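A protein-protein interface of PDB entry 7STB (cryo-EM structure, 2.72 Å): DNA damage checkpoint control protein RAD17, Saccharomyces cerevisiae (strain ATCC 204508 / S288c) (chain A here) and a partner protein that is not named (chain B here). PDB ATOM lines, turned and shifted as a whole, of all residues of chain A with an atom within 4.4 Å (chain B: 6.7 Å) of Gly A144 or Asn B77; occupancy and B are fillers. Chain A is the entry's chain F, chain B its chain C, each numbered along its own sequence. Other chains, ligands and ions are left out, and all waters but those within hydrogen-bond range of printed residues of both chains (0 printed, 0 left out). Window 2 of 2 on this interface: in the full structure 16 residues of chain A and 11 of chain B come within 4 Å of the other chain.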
ATOM      1  N   PHE A 140      12.869  24.351 -10.641  1.00  0.00           N
ATOM      2  CA  PHE A 140      11.913  23.287 -10.371  1.00  0.00           C
ATOM      3  C   PHE A 140      11.795  23.059  -8.870  1.00  0.00           C
ATOM      4  O   PHE A 140      12.801  22.947  -8.164  1.00  0.00           O
ATOM      5  CB  PHE A 140      12.352  22.000 -11.071  1.00  0.00           C
ATOM      6  CG  PHE A 140      11.504  20.804 -10.737  1.00  0.00           C
ATOM      7  CD1 PHE A 140      10.362  20.523 -11.469  1.00  0.00           C
ATOM      8  CD2 PHE A 140      11.853  19.957  -9.698  1.00  0.00           C
ATOM      9  CE1 PHE A 140       9.581  19.423 -11.167  1.00  0.00           C
ATOM     10  CE2 PHE A 140      11.075  18.856  -9.391  1.00  0.00           C
ATOM     11  CZ  PHE A 140       9.939  18.589 -10.127  1.00  0.00           C
ATOM     12  N   ASP A 141      10.558  22.992  -8.384  1.00  0.00           N
ATOM     13  CA  ASP A 141      10.285  22.750  -6.971  1.00  0.00           C
ATOM     14  C   ASP A 141      10.136  21.249  -6.758  1.00  0.00           C
ATOM     15  O   ASP A 141       9.200  20.630  -7.275  1.00  0.00           O
ATOM     16  CB  ASP A 141       9.029  23.496  -6.530  1.00  0.00           C
ATOM     17  CG  ASP A 141       8.553  23.074  -5.154  1.00  0.00           C
ATOM     18  OD1 ASP A 141       9.398  22.955  -4.242  1.00  0.00           O
ATOM     19  OD2 ASP A 141       7.334  22.860  -4.986  1.00  0.00           O
ATOM     20  N   THR A 142      11.058  20.662  -5.993  1.00  0.00           N
ATOM     21  CA  THR A 142      10.993  19.236  -5.700  1.00  0.00           C
ATOM     22  C   THR A 142       9.825  18.879  -4.791  1.00  0.00           C
ATOM     23  O   THR A 142       9.523  17.690  -4.640  1.00  0.00           O
ATOM     24  CB  THR A 142      12.302  18.771  -5.058  1.00  0.00           C
ATOM     25  OG1 THR A 142      12.296  17.343  -4.933  1.00  0.00           O
ATOM     26  CG2 THR A 142      12.484  19.398  -3.681  1.00  0.00           C
ATOM     27  N   ASN A 143       9.169  19.867  -4.187  1.00  0.00           N
ATOM     28  CA  ASN A 143       8.024  19.634  -3.318  1.00  0.00           C
ATOM     29  C   ASN A 143       6.699  19.637  -4.070  1.00  0.00           C
ATOM     30  O   ASN A 143       5.646  19.519  -3.436  1.00  0.00           O
ATOM     31  CB  ASN A 143       7.983  20.693  -2.211  1.00  0.00           C
ATOM     32  CG  ASN A 143       9.135  20.559  -1.234  1.00  0.00           C
ATOM     33  OD1 ASN A 143       9.844  19.553  -1.226  1.00  0.00           O
ATOM     34  ND2 ASN A 143       9.326  21.577  -0.402  1.00  0.00           N
ATOM     35  N   GLY A 144       6.725  19.773  -5.398  1.00  0.00           N
ATOM     36  CA  GLY A 144       5.493  19.798  -6.166  1.00  0.00           C
ATOM     37  C   GLY A 144       4.741  18.484  -6.169  1.00  0.00           C
ATOM     38  O   GLY A 144       3.522  18.480  -6.372  1.00  0.00           O
ATOM     39  N   LEU A 145       5.435  17.370  -5.950  1.00  0.00           N
ATOM     40  CA  LEU A 145       4.821  16.047  -5.925  1.00  0.00           C
ATOM     41  C   LEU A 145       4.561  15.660  -4.474  1.00  0.00           C
ATOM     42  O   LEU A 145       5.502  15.468  -3.698  1.00  0.00           O
ATOM     43  CB  LEU A 145       5.719  15.023  -6.616  1.00  0.00           C
ATOM     44  CG  LEU A 145       5.174  13.598  -6.725  1.00  0.00           C
ATOM     45  CD1 LEU A 145       3.908  13.560  -7.565  1.00  0.00           C
ATOM     46  CD2 LEU A 145       6.230  12.672  -7.309  1.00  0.00           C
ATOM     47  N   GLU A 146       3.284  15.549  -4.111  1.00  0.00           N
ATOM     48  CA  GLU A 146       2.903  15.174  -2.758  1.00  0.00           C
ATOM     49  C   GLU A 146       1.561  14.460  -2.801  1.00  0.00           C
ATOM     50  O   GLU A 146       0.829  14.529  -3.792  1.00  0.00           O
ATOM     51  CB  GLU A 146       2.836  16.394  -1.827  1.00  0.00           C
ATOM     52  CG  GLU A 146       1.759  17.415  -2.183  1.00  0.00           C
ATOM     53  CD  GLU A 146       2.274  18.523  -3.079  1.00  0.00           C
ATOM     54  OE1 GLU A 146       3.357  18.352  -3.673  1.00  0.00           O
ATOM     55  OE2 GLU A 146       1.596  19.565  -3.188  1.00  0.00           O
ATOM     56  N   LYS B  73       1.687  28.617 -10.220  1.00  0.00           N
ATOM     57  CA  LYS B  73       2.802  28.250  -9.357  1.00  0.00           C
ATOM     58  C   LYS B  73       3.261  26.810  -9.554  1.00  0.00           C
ATOM     59  O   LYS B  73       4.301  26.430  -9.006  1.00  0.00           O
ATOM     60  CB  LYS B  73       2.421  28.459  -7.887  1.00  0.00           C
ATOM     61  CG  LYS B  73       2.235  29.915  -7.495  1.00  0.00           C
ATOM     62  CD  LYS B  73       1.913  30.053  -6.016  1.00  0.00           C
ATOM     63  CE  LYS B  73       1.720  31.508  -5.619  1.00  0.00           C
ATOM     64  NZ  LYS B  73       1.379  31.654  -4.177  1.00  0.00           N
ATOM     65  N   ASN B  74       2.524  26.008 -10.317  1.00  0.00           N
ATOM     66  CA  ASN B  74       2.876  24.618 -10.563  1.00  0.00           C
ATOM     67  C   ASN B  74       3.735  24.439 -11.809  1.00  0.00           C
ATOM     68  O   ASN B  74       4.070  23.303 -12.158  1.00  0.00           O
ATOM     69  CB  ASN B  74       1.606  23.770 -10.685  1.00  0.00           C
ATOM     70  CG  ASN B  74       0.690  23.916  -9.486  1.00  0.00           C
ATOM     71  OD1 ASN B  74       0.971  24.683  -8.565  1.00  0.00           O
ATOM     72  ND2 ASN B  74      -0.414  23.179  -9.493  1.00  0.00           N
ATOM     73  N   TYR B  75       4.111  25.536 -12.475  1.00  0.00           N
ATOM     74  CA  TYR B  75       4.871  25.445 -13.718  1.00  0.00           C
ATOM     75  C   TYR B  75       6.063  24.505 -13.606  1.00  0.00           C
ATOM     76  O   TYR B  75       6.504  23.938 -14.613  1.00  0.00           O
ATOM     77  CB  TYR B  75       5.345  26.838 -14.136  1.00  0.00           C
ATOM     78  CG  TYR B  75       6.337  26.830 -15.276  1.00  0.00           C
ATOM     79  CD1 TYR B  75       5.928  26.593 -16.578  1.00  0.00           C
ATOM     80  CD2 TYR B  75       7.687  27.059 -15.046  1.00  0.00           C
ATOM     81  CE1 TYR B  75       6.833  26.582 -17.621  1.00  0.00           C
ATOM     82  CE2 TYR B  75       8.599  27.051 -16.082  1.00  0.00           C
ATOM     83  CZ  TYR B  75       8.167  26.812 -17.367  1.00  0.00           C
ATOM     84  OH  TYR B  75       9.073  26.803 -18.402  1.00  0.00           O
ATOM     85  N   SER B  76       6.602  24.324 -12.399  1.00  0.00           N
ATOM     86  CA  SER B  76       7.783  23.482 -12.235  1.00  0.00           C
ATOM     87  C   SER B  76       7.504  22.046 -12.662  1.00  0.00           C
ATOM     88  O   SER B  76       8.239  21.475 -13.475  1.00  0.00           O
ATOM     89  CB  SER B  76       8.252  23.526 -10.783  1.00  0.00           C
ATOM     90  OG  SER B  76       8.787  24.798 -10.456  1.00  0.00           O
ATOM     91  N   ASN B  77       6.444  21.445 -12.125  1.00  0.00           N
ATOM     92  CA  ASN B  77       6.138  20.041 -12.365  1.00  0.00           C
ATOM     93  C   ASN B  77       5.031  19.823 -13.389  1.00  0.00           C
ATOM     94  O   ASN B  77       4.673  18.670 -13.652  1.00  0.00           O
ATOM     95  CB  ASN B  77       5.771  19.355 -11.043  1.00  0.00           C
ATOM     96  CG  ASN B  77       4.513  19.923 -10.416  1.00  0.00           C
ATOM     97  OD1 ASN B  77       3.827  20.752 -11.010  1.00  0.00           O
ATOM     98  ND2 ASN B  77       4.203  19.474  -9.206  1.00  0.00           N
ATOM     99  N   MET B  78       4.480  20.888 -13.972  1.00  0.00           N
ATOM    100  CA  MET B  78       3.486  20.746 -15.028  1.00  0.00           C
ATOM    101  C   MET B  78       4.084  20.827 -16.424  1.00  0.00           C
ATOM    102  O   MET B  78       3.423  20.427 -17.388  1.00  0.00           O
ATOM    103  CB  MET B  78       2.405  21.827 -14.899  1.00  0.00           C
ATOM    104  CG  MET B  78       1.657  21.865 -13.570  1.00  0.00           C
ATOM    105  SD  MET B  78       1.536  20.296 -12.691  1.00  0.00           S
ATOM    106  CE  MET B  78       0.582  19.324 -13.850  1.00  0.00           C
ATOM    107  N   VAL B  79       5.308  21.332 -16.559  1.00  0.00           N
ATOM    108  CA  VAL B  79       5.927  21.578 -17.856  1.00  0.00           C
ATOM    109  C   VAL B  79       7.308  20.941 -17.870  1.00  0.00           C
ATOM    110  O   VAL B  79       8.065  21.066 -16.902  1.00  0.00           O
ATOM    111  CB  VAL B  79       6.027  23.085 -18.160  1.00  0.00           C
ATOM    112  CG1 VAL B  79       6.751  23.319 -19.479  1.00  0.00           C
ATOM    113  CG2 VAL B  79       4.643  23.709 -18.182  1.00  0.00           C
ATOM    114  N   LEU B  80       7.630  20.258 -18.966  1.00  0.00           N
ATOM    115  CA  LEU B  80       8.954  19.687 -19.185  1.00  0.00           C
ATOM    116  C   LEU B  80       9.601  20.420 -20.353  1.00  0.00           C
ATOM    117  O   LEU B  80       9.097  20.364 -21.478  1.00  0.00           O
ATOM    118  CB  LEU B  80       8.861  18.186 -19.466  1.00  0.00           C
ATOM    119  CG  LEU B  80      10.146  17.469 -19.892  1.00  0.00           C
ATOM    120  CD1 LEU B  80      11.011  17.166 -18.680  1.00  0.00           C
ATOM    121  CD2 LEU B  80       9.820  16.193 -20.650  1.00  0.00           C
ATOM    122  N   PHE B 100       7.438  11.077 -19.192  1.00  0.00           N
ATOM    123  CA  PHE B 100       6.716  12.273 -18.772  1.00  0.00           C
ATOM    124  C   PHE B 100       5.320  12.322 -19.380  1.00  0.00           C
ATOM    125  O   PHE B 100       4.349  12.663 -18.695  1.00  0.00           O
ATOM    126  CB  PHE B 100       7.500  13.529 -19.149  1.00  0.00           C
ATOM    127  CG  PHE B 100       6.887  14.798 -18.628  1.00  0.00           C
ATOM    128  CD1 PHE B 100       6.794  15.030 -17.265  1.00  0.00           C
ATOM    129  CD2 PHE B 100       6.402  15.757 -19.499  1.00  0.00           C
ATOM    130  CE1 PHE B 100       6.229  16.194 -16.783  1.00  0.00           C
ATOM    131  CE2 PHE B 100       5.835  16.923 -19.022  1.00  0.00           C
ATOM    132  CZ  PHE B 100       5.749  17.142 -17.663  1.00  0.00           C
ATOM    133  N   GLN B 105      -1.800  13.218 -14.063  1.00  0.00           N
ATOM    134  CA  GLN B 105      -1.624  14.617 -13.710  1.00  0.00           C
ATOM    135  C   GLN B 105      -1.544  14.781 -12.197  1.00  0.00           C
ATOM    136  O   GLN B 105      -2.151  14.022 -11.438  1.00  0.00           O
ATOM    137  CB  GLN B 105      -2.778  15.455 -14.260  1.00  0.00           C
ATOM    138  CG  GLN B 105      -2.437  16.917 -14.433  1.00  0.00           C
ATOM    139  CD  GLN B 105      -1.516  17.141 -15.611  1.00  0.00           C
ATOM    140  OE1 GLN B 105      -0.301  17.244 -15.453  1.00  0.00           O
ATOM    141  NE2 GLN B 105      -2.090  17.207 -16.804  1.00  0.00           N
ATOM    142  N   ILE B 106      -0.780  15.787 -11.765  1.00  0.00           N
ATOM    143  CA  ILE B 106      -0.638  16.048 -10.336  1.00  0.00           C
ATOM    144  C   ILE B 106      -1.952  16.555  -9.754  1.00  0.00           C
ATOM    145  O   ILE B 106      -2.409  16.085  -8.705  1.00  0.00           O
ATOM    146  CB  ILE B 106       0.506  17.046 -10.080  1.00  0.00           C
ATOM    147  CG1 ILE B 106       1.784  16.609 -10.802  1.00  0.00           C
ATOM    148  CG2 ILE B 106       0.762  17.187  -8.586  1.00  0.00           C
ATOM    149  CD1 ILE B 106       2.219  15.194 -10.488  1.00  0.00           C
ATOM    150  N   PHE B 107      -2.582  17.522 -10.428  1.00  0.00           N
ATOM    151  CA  PHE B 107      -3.823  18.122  -9.950  1.00  0.00           C
ATOM    152  C   PHE B 107      -4.845  18.285 -11.069  1.00  0.00           C
ATOM    153  O   PHE B 107      -5.723  19.149 -10.977  1.00  0.00           O
ATOM    154  CB  PHE B 107      -3.547  19.477  -9.292  1.00  0.00           C
ATOM    155  CG  PHE B 107      -2.771  19.383  -8.009  1.00  0.00           C
ATOM    156  CD1 PHE B 107      -3.283  18.694  -6.922  1.00  0.00           C
ATOM    157  CD2 PHE B 107      -1.531  19.987  -7.888  1.00  0.00           C
ATOM    158  CE1 PHE B 107      -2.571  18.607  -5.740  1.00  0.00           C
ATOM    159  CE2 PHE B 107      -0.815  19.904  -6.709  1.00  0.00           C
ATOM    160  CZ  PHE B 107      -1.336  19.213  -5.634  1.00  0.00           C
ATOM    161  N   LYS B 112      -0.296  18.216 -19.670  1.00  0.00           N
ATOM    162  CA  LYS B 112       1.132  18.387 -19.445  1.00  0.00           C
ATOM    163  C   LYS B 112       1.768  18.941 -20.710  1.00  0.00           C
ATOM    164  O   LYS B 112       1.534  18.422 -21.805  1.00  0.00           O
ATOM    165  CB  LYS B 112       1.790  17.060 -19.058  1.00  0.00           C
ATOM    166  CG  LYS B 112       1.172  16.397 -17.840  1.00  0.00           C
ATOM    167  CD  LYS B 112       1.674  14.974 -17.654  1.00  0.00           C
ATOM    168  CE  LYS B 112       3.054  14.944 -17.025  1.00  0.00           C
ATOM    169  NZ  LYS B 112       3.432  13.573 -16.588  1.00  0.00           N
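Ser B76 touches Phe A140 (O to CD1, 3.1 Å).
CE1 of Phe A140 touches CA of Asn B77, at 3.7 Å.
Ile B106 touches Gly A144.
Ile B106 touches Leu A145.
OE2 of Glu A146 touches CZ of Phe B107, 3.8 Å away.
OG of Ser B76 sits at hydrogen-bond distance from N of Asp A141 (3.3 Å).
The side-chain amide nitrogen (ND2) of Asn B77 lies within hydrogen-bond range of the backbone carbonyl oxygen (O) of Gly A144 (3.1 Å).
Hydrophobic or aromatic side chains of chain B within 4 Å of the printed part of chain A: Ile B106 and Phe B107.
Of the 7 printed residues of chain A, 5 touch a printed residue of chain B.
Among the printed residues, 7 pairs touch across the chains.
Among the printed residues, no Asp or Glu carboxylate lies within 4 Å of a Lys or Arg side-chain nitrogen of the other chain.
The backbone carbonyl oxygen (O) of Asn B74 sits close to the side-chain amide oxygen (OD1) of Asn B77 (2.8 Å).
The side-chain sulfur (SD) of Met B78 sits close to the side-chain amide oxygen (OD1) of Asn B77.
The side-chain carboxylate (OD1) of Asp A141 sits close to the backbone NH (N) of Asn A143 (3.1 Å).
The side-chain carboxylate (OD2) of Asp A141 is in hydrogen-bond range of the backbone NH (N) of Gly A144, at 3.2 Å.
OE1 of Glu A146 lies close to O of Asn A143, at 2.6 Å.
The side-chain carboxylate of Glu A146 lies close to the backbone carbonyl oxygen of Gly A144 (2.7 Å).
Gly A144 touches just these residues of chain B: Asn B77 (3.1 Å) and Ile B106 (3.8 Å).
Of the printed residues of chain A, Ser B76 touches Phe A140 (3.1 Å) and Asp A141 (3.3 Å).
Of the printed residues of chain B, Asp A141 touches Ser B76.
Of the printed residues of chain B, Phe A140 touches Ser B76 (3.1 Å) and Asn B77 (3.7 Å).
Printed residues of chain B within 4 Å of Leu A145: Ile B106 (3.8 Å).
The nearest residue of chain A that does not touch Asn B77 is Leu A145 (4.1 Å).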
